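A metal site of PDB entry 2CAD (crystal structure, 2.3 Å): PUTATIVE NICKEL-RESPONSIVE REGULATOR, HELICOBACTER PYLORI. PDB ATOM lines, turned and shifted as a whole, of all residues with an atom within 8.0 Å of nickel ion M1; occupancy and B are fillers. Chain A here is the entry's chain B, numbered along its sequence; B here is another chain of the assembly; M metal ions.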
ATOM      1  N   TYR A  72     -25.659   1.029 -12.044  1.00  0.00           N
ATOM      2  CA  TYR A  72     -24.931   1.208 -13.286  1.00  0.00           C
ATOM      3  C   TYR A  72     -25.664   0.642 -14.520  1.00  0.00           C
ATOM      4  O   TYR A  72     -26.584  -0.188 -14.397  1.00  0.00           O
ATOM      5  CB  TYR A  72     -23.513   0.681 -13.162  1.00  0.00           C
ATOM      6  CG  TYR A  72     -23.354  -0.828 -13.128  1.00  0.00           C
ATOM      7  CD1 TYR A  72     -23.077  -1.543 -14.295  1.00  0.00           C
ATOM      8  CD2 TYR A  72     -23.440  -1.536 -11.934  1.00  0.00           C
ATOM      9  CE1 TYR A  72     -22.924  -2.924 -14.260  1.00  0.00           C
ATOM     10  CE2 TYR A  72     -23.287  -2.879 -11.897  1.00  0.00           C
ATOM     11  CZ  TYR A  72     -23.033  -3.586 -13.060  1.00  0.00           C
ATOM     12  OH  TYR A  72     -22.842  -4.949 -12.995  1.00  0.00           O
ATOM     13  N   ASP A  73     -25.259   1.150 -15.690  1.00  0.00           N
ATOM     14  CA  ASP A  73     -25.788   0.785 -17.019  1.00  0.00           C
ATOM     15  C   ASP A  73     -24.959  -0.388 -17.558  1.00  0.00           C
ATOM     16  O   ASP A  73     -23.771  -0.263 -17.838  1.00  0.00           O
ATOM     17  CB  ASP A  73     -25.650   2.013 -17.956  1.00  0.00           C
ATOM     18  CG  ASP A  73     -26.372   1.837 -19.313  1.00  0.00           C
ATOM     19  OD1 ASP A  73     -27.059   0.825 -19.591  1.00  0.00           O
ATOM     20  OD2 ASP A  73     -26.244   2.779 -20.110  1.00  0.00           O
ATOM     21  N   HIS A  74     -25.579  -1.562 -17.680  1.00  0.00           N
ATOM     22  CA  HIS A  74     -24.838  -2.743 -18.140  1.00  0.00           C
ATOM     23  C   HIS A  74     -24.538  -2.672 -19.643  1.00  0.00           C
ATOM     24  O   HIS A  74     -23.716  -3.449 -20.144  1.00  0.00           O
ATOM     25  CB  HIS A  74     -25.575  -4.026 -17.813  1.00  0.00           C
ATOM     26  CG  HIS A  74     -26.644  -4.384 -18.797  1.00  0.00           C
ATOM     27  ND1 HIS A  74     -26.435  -5.328 -19.788  1.00  0.00           N
ATOM     28  CD2 HIS A  74     -27.910  -3.958 -18.941  1.00  0.00           C
ATOM     29  CE1 HIS A  74     -27.545  -5.463 -20.496  1.00  0.00           C
ATOM     30  NE2 HIS A  74     -28.451  -4.644 -20.008  1.00  0.00           N
ATOM     31  N   HIS A  99     -26.581  -8.841  -7.210  1.00  0.00           N
ATOM     32  CA  HIS A  99     -26.903  -8.015  -8.369  1.00  0.00           C
ATOM     33  C   HIS A  99     -28.361  -8.160  -8.661  1.00  0.00           C
ATOM     34  O   HIS A  99     -28.863  -9.284  -8.706  1.00  0.00           O
ATOM     35  CB  HIS A  99     -26.044  -8.481  -9.542  1.00  0.00           C
ATOM     36  CG  HIS A  99     -26.237  -7.742 -10.833  1.00  0.00           C
ATOM     37  ND1 HIS A  99     -25.204  -7.041 -11.433  1.00  0.00           N
ATOM     38  CD2 HIS A  99     -27.279  -7.707 -11.709  1.00  0.00           C
ATOM     39  CE1 HIS A  99     -25.627  -6.562 -12.592  1.00  0.00           C
ATOM     40  NE2 HIS A  99     -26.886  -6.942 -12.782  1.00  0.00           N
ATOM     41  N   ILE A 100     -29.051  -7.045  -8.840  1.00  0.00           N
ATOM     42  CA  ILE A 100     -30.448  -7.018  -9.286  1.00  0.00           C
ATOM     43  C   ILE A 100     -30.513  -6.396 -10.675  1.00  0.00           C
ATOM     44  O   ILE A 100     -29.977  -5.322 -10.896  1.00  0.00           O
ATOM     45  CB  ILE A 100     -31.365  -6.215  -8.339  1.00  0.00           C
ATOM     46  CG1 ILE A 100     -31.377  -6.804  -6.935  1.00  0.00           C
ATOM     47  CG2 ILE A 100     -32.774  -6.169  -8.887  1.00  0.00           C
ATOM     48  CD1 ILE A 100     -32.261  -8.010  -6.778  1.00  0.00           C
ATOM     49  N   HIS A 101     -31.132  -7.078 -11.629  1.00  0.00           N
ATOM     50  CA  HIS A 101     -31.324  -6.512 -12.964  1.00  0.00           C
ATOM     51  C   HIS A 101     -32.584  -5.678 -12.924  1.00  0.00           C
ATOM     52  O   HIS A 101     -33.671  -6.174 -13.208  1.00  0.00           O
ATOM     53  CB  HIS A 101     -31.414  -7.605 -14.057  1.00  0.00           C
ATOM     54  CG  HIS A 101     -30.346  -8.658 -13.993  1.00  0.00           C
ATOM     55  ND1 HIS A 101     -29.007  -8.373 -14.167  1.00  0.00           N
ATOM     56  CD2 HIS A 101     -30.424  -9.992 -13.834  1.00  0.00           C
ATOM     57  CE1 HIS A 101     -28.309  -9.492 -14.077  1.00  0.00           C
ATOM     58  NE2 HIS A 101     -29.155 -10.487 -13.858  1.00  0.00           N
ATOM     59  N   MET A 102     -32.429  -4.402 -12.548  1.00  0.00           N
ATOM     60  CA  MET A 102     -33.571  -3.509 -12.286  1.00  0.00           C
ATOM     61  C   MET A 102     -34.435  -3.266 -13.551  1.00  0.00           C
ATOM     62  O   MET A 102     -35.631  -3.434 -13.519  1.00  0.00           O
ATOM     63  CB  MET A 102     -33.086  -2.146 -11.745  1.00  0.00           C
ATOM     64  CG  MET A 102     -32.380  -2.084 -10.361  1.00  0.00           C
ATOM     65  SD  MET A 102     -31.548  -0.442 -10.106  1.00  0.00           S
ATOM     66  CE  MET A 102     -32.965   0.630  -9.853  1.00  0.00           C
ATOM     67  N   ASP A 103     -33.807  -2.853 -14.647  1.00  0.00           N
ATOM     68  CA  ASP A 103     -34.490  -2.646 -15.927  1.00  0.00           C
ATOM     69  C   ASP A 103     -33.472  -2.777 -17.064  1.00  0.00           C
ATOM     70  O   ASP A 103     -32.409  -3.389 -16.888  1.00  0.00           O
ATOM     71  CB  ASP A 103     -35.250  -1.307 -15.960  1.00  0.00           C
ATOM     72  CG  ASP A 103     -34.349  -0.097 -15.820  1.00  0.00           C
ATOM     73  OD1 ASP A 103     -33.356   0.044 -16.564  1.00  0.00           O
ATOM     74  OD2 ASP A 103     -34.632   0.737 -14.940  1.00  0.00           O
ATOM     75  N   GLU A 104     -33.788  -2.176 -18.217  1.00  0.00           N
ATOM     76  CA  GLU A 104     -33.076  -2.460 -19.467  1.00  0.00           C
ATOM     77  C   GLU A 104     -31.664  -1.967 -19.397  1.00  0.00           C
ATOM     78  O   GLU A 104     -30.756  -2.556 -19.975  1.00  0.00           O
ATOM     79  CB  GLU A 104     -33.783  -1.830 -20.682  1.00  0.00           C
ATOM     80  CG  GLU A 104     -35.266  -2.256 -20.871  1.00  0.00           C
ATOM     81  CD  GLU A 104     -36.221  -1.560 -19.894  1.00  0.00           C
ATOM     82  OE1 GLU A 104     -36.141  -0.321 -19.765  1.00  0.00           O
ATOM     83  OE2 GLU A 104     -37.042  -2.255 -19.248  1.00  0.00           O
ATOM     84  N   HIS A 105     -31.458  -0.869 -18.675  1.00  0.00           N
ATOM     85  CA  HIS A 105     -30.123  -0.373 -18.445  1.00  0.00           C
ATOM     86  C   HIS A 105     -29.577  -0.705 -17.042  1.00  0.00           C
ATOM     87  O   HIS A 105     -28.527  -1.387 -16.909  1.00  0.00           O
ATOM     88  CB  HIS A 105     -30.104   1.121 -18.756  1.00  0.00           C
ATOM     89  CG  HIS A 105     -30.092   1.397 -20.223  1.00  0.00           C
ATOM     90  ND1 HIS A 105     -28.918   1.539 -20.933  1.00  0.00           N
ATOM     91  CD2 HIS A 105     -31.091   1.456 -21.122  1.00  0.00           C
ATOM     92  CE1 HIS A 105     -29.197   1.710 -22.208  1.00  0.00           C
ATOM     93  NE2 HIS A 105     -30.507   1.667 -22.355  1.00  0.00           N
ATOM     94  N   ASN A 106     -30.331  -0.297 -16.025  1.00  0.00           N
ATOM     95  CA  ASN A 106     -29.882  -0.247 -14.622  1.00  0.00           C
ATOM     96  C   ASN A 106     -29.742  -1.604 -13.956  1.00  0.00           C
ATOM     97  O   ASN A 106     -30.684  -2.384 -13.944  1.00  0.00           O
ATOM     98  CB  ASN A 106     -30.832   0.602 -13.767  1.00  0.00           C
ATOM     99  CG  ASN A 106     -31.011   2.003 -14.301  1.00  0.00           C
ATOM    100  OD1 ASN A 106     -30.070   2.790 -14.306  1.00  0.00           O
ATOM    101  ND2 ASN A 106     -32.209   2.308 -14.779  1.00  0.00           N
ATOM    102  N   CYS A 107     -28.545  -1.834 -13.427  1.00  0.00           N
ATOM    103  CA  CYS A 107     -28.189  -2.888 -12.507  1.00  0.00           C
ATOM    104  C   CYS A 107     -27.839  -2.227 -11.163  1.00  0.00           C
ATOM    105  O   CYS A 107     -27.187  -1.197 -11.130  1.00  0.00           O
ATOM    106  CB  CYS A 107     -26.937  -3.610 -12.997  1.00  0.00           C
ATOM    107  SG  CYS A 107     -27.131  -4.435 -14.600  1.00  0.00           S
ATOM    108  N   LEU A 108     -28.312  -2.825 -10.079  1.00  0.00           N
ATOM    109  CA  LEU A 108     -27.908  -2.486  -8.747  1.00  0.00           C
ATOM    110  C   LEU A 108     -27.132  -3.649  -8.187  1.00  0.00           C
ATOM    111  O   LEU A 108     -27.546  -4.795  -8.354  1.00  0.00           O
ATOM    112  CB  LEU A 108     -29.133  -2.208  -7.873  1.00  0.00           C
ATOM    113  CG  LEU A 108     -28.765  -1.657  -6.473  1.00  0.00           C
ATOM    114  CD1 LEU A 108     -29.801  -0.700  -6.008  1.00  0.00           C
ATOM    115  CD2 LEU A 108     -28.587  -2.749  -5.478  1.00  0.00           C
ATOM    116  N   GLU A 109     -26.003  -3.358  -7.556  1.00  0.00           N
ATOM    117  CA  GLU A 109     -25.206  -4.341  -6.849  1.00  0.00           C
ATOM    118  C   GLU A 109     -24.927  -3.887  -5.450  1.00  0.00           C
ATOM    119  O   GLU A 109     -24.711  -2.736  -5.231  1.00  0.00           O
ATOM    120  CB  GLU A 109     -23.874  -4.592  -7.524  1.00  0.00           C
ATOM    121  CG  GLU A 109     -24.014  -5.292  -8.801  1.00  0.00           C
ATOM    122  CD  GLU A 109     -22.696  -5.546  -9.519  1.00  0.00           C
ATOM    123  OE1 GLU A 109     -21.622  -5.090  -9.047  1.00  0.00           O
ATOM    124  OE2 GLU A 109     -22.781  -6.232 -10.571  1.00  0.00           O
ATOM    125  N   MET B  83     -22.306 -12.769 -18.942  1.00  0.00           N
ATOM    126  CA  MET B  83     -23.417 -13.370 -18.142  1.00  0.00           C
ATOM    127  C   MET B  83     -24.522 -12.361 -17.810  1.00  0.00           C
ATOM    128  O   MET B  83     -25.710 -12.652 -17.943  1.00  0.00           O
ATOM    129  CB  MET B  83     -22.869 -14.000 -16.865  1.00  0.00           C
ATOM    130  CG  MET B  83     -21.958 -15.205 -17.121  1.00  0.00           C
ATOM    131  SD  MET B  83     -21.717 -16.271 -15.696  1.00  0.00           S
ATOM    132  CE  MET B  83     -20.617 -15.321 -14.717  1.00  0.00           C
ATOM    133  N   ILE B  84     -24.128 -11.141 -17.436  1.00  0.00           N
ATOM    134  CA  ILE B  84     -25.102 -10.071 -17.117  1.00  0.00           C
ATOM    135  C   ILE B  84     -25.916  -9.725 -18.345  1.00  0.00           C
ATOM    136  O   ILE B  84     -27.144  -9.660 -18.284  1.00  0.00           O
ATOM    137  CB  ILE B  84     -24.384  -8.821 -16.557  1.00  0.00           C
ATOM    138  CG1 ILE B  84     -23.847  -9.135 -15.146  1.00  0.00           C
ATOM    139  CG2 ILE B  84     -25.324  -7.616 -16.525  1.00  0.00           C
ATOM    140  CD1 ILE B  84     -22.787  -8.176 -14.670  1.00  0.00           C
ATOM    141  N   ASP B  85     -25.235  -9.508 -19.465  1.00  0.00           N
ATOM    142  CA  ASP B  85     -25.943  -9.272 -20.722  1.00  0.00           C
ATOM    143  C   ASP B  85     -26.948 -10.374 -21.050  1.00  0.00           C
ATOM    144  O   ASP B  85     -28.114 -10.087 -21.394  1.00  0.00           O
ATOM    145  CB  ASP B  85     -24.965  -9.099 -21.884  1.00  0.00           C
ATOM    146  CG  ASP B  85     -24.202  -7.785 -21.821  1.00  0.00           C
ATOM    147  OD1 ASP B  85     -24.571  -6.865 -21.039  1.00  0.00           O
ATOM    148  OD2 ASP B  85     -23.203  -7.684 -22.533  1.00  0.00           O
ATOM    149  N   GLN B  87     -28.381 -12.535 -19.040  1.00  0.00           N
ATOM    150  CA  GLN B  87     -29.449 -12.479 -18.040  1.00  0.00           C
ATOM    151  C   GLN B  87     -30.415 -11.371 -18.348  1.00  0.00           C
ATOM    152  O   GLN B  87     -31.641 -11.574 -18.277  1.00  0.00           O
ATOM    153  CB  GLN B  87     -28.844 -12.309 -16.640  1.00  0.00           C
ATOM    154  CG  GLN B  87     -28.186 -13.583 -16.146  1.00  0.00           C
ATOM    155  CD  GLN B  87     -27.455 -13.396 -14.849  1.00  0.00           C
ATOM    156  OE1 GLN B  87     -28.036 -12.925 -13.858  1.00  0.00           O
ATOM    157  NE2 GLN B  87     -26.169 -13.791 -14.818  1.00  0.00           N
ATOM    158  N   HIS B  88     -29.875 -10.188 -18.670  1.00  0.00           N
ATOM    159  CA  HIS B  88     -30.691  -9.048 -19.143  1.00  0.00           C
ATOM    160  C   HIS B  88     -31.453  -9.352 -20.429  1.00  0.00           C
ATOM    161  O   HIS B  88     -32.662  -9.071 -20.501  1.00  0.00           O
ATOM    162  CB  HIS B  88     -29.841  -7.779 -19.332  1.00  0.00           C
ATOM    163  CG  HIS B  88     -29.638  -7.004 -18.062  1.00  0.00           C
ATOM    164  ND1 HIS B  88     -30.319  -5.844 -17.759  1.00  0.00           N
ATOM    165  CD2 HIS B  88     -28.828  -7.246 -16.992  1.00  0.00           C
ATOM    166  CE1 HIS B  88     -29.948  -5.407 -16.582  1.00  0.00           C
ATOM    167  NE2 HIS B  88     -29.051  -6.238 -16.095  1.00  0.00           N
ATOM    168  N   VAL B  94     -35.082 -12.682 -14.242  1.00  0.00           N
ATOM    169  CA  VAL B  94     -34.040 -12.992 -13.286  1.00  0.00           C
ATOM    170  C   VAL B  94     -34.264 -12.086 -12.077  1.00  0.00           C
ATOM    171  O   VAL B  94     -34.286 -10.867 -12.201  1.00  0.00           O
ATOM    172  CB  VAL B  94     -32.629 -12.815 -13.888  1.00  0.00           C
ATOM    173  CG1 VAL B  94     -31.541 -13.021 -12.818  1.00  0.00           C
ATOM    174  CG2 VAL B  94     -32.415 -13.799 -15.034  1.00  0.00           C
ATOM    175  N   THR B  97     -28.989 -12.372  -8.584  1.00  0.00           N
ATOM    176  CA  THR B  97     -27.768 -13.112  -8.741  1.00  0.00           C
ATOM    177  C   THR B  97     -26.894 -12.816  -7.545  1.00  0.00           C
ATOM    178  O   THR B  97     -26.859 -11.687  -7.067  1.00  0.00           O
ATOM    179  CB  THR B  97     -27.050 -12.693 -10.040  1.00  0.00           C
ATOM    180  OG1 THR B  97     -27.864 -13.097 -11.146  1.00  0.00           O
ATOM    181  CG2 THR B  97     -25.788 -13.386 -10.155  1.00  0.00           C
HETATM  182 NI    NI M   1     -28.080  -6.497 -14.327  1.00  0.00          NI
HETATM  183 NI    NI M   2     -30.078  -3.989 -21.175  1.00  0.00          NI
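ND1 of His 99 lies within hydrogen-bond range of OE2 of Glu 109. The backbone NH (N) of His 99 lies within hydrogen-bond range of the backbone carbonyl oxygen (O) of Thr 97 of chain B, at 2.9 Å. A ring nitrogen (ND1) of His 88 of chain B lies close to a ring nitrogen (NE2) of His 74, 3.2 Å away. A ring nitrogen (ND1) of His 88 of chain B lies close to the backbone carbonyl oxygen of Asp 103 (3.3 Å). A ring nitrogen (NE2) of His 101 lies within hydrogen-bond range of the side-chain amide oxygen (OE1) of Gln 87 of chain B (2.7 Å). The backbone carbonyl oxygen of Tyr 72 sits at hydrogen-bond distance from the backbone NH of Cys 107, 2.7 Å away.
Nickel ion M1 is bound by NE2 of His 99, 2.0 Å away. NE2 of His 88 of chain B binds nickel ion M1 (2.0 Å). ND1 of His 101 is bound to nickel ion M1 (2.1 Å). Nickel ion M1 is bound by SG of Cys 107 (2.3 Å). Nickel ion M1 has four donor atoms within binding distance.
Merely in contact with nickel ion M1: Ile 84 of chain B (3.7 Å). The nearest printed residue that does not touch nickel ion M1 is Ile 100 (4.1 Å).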
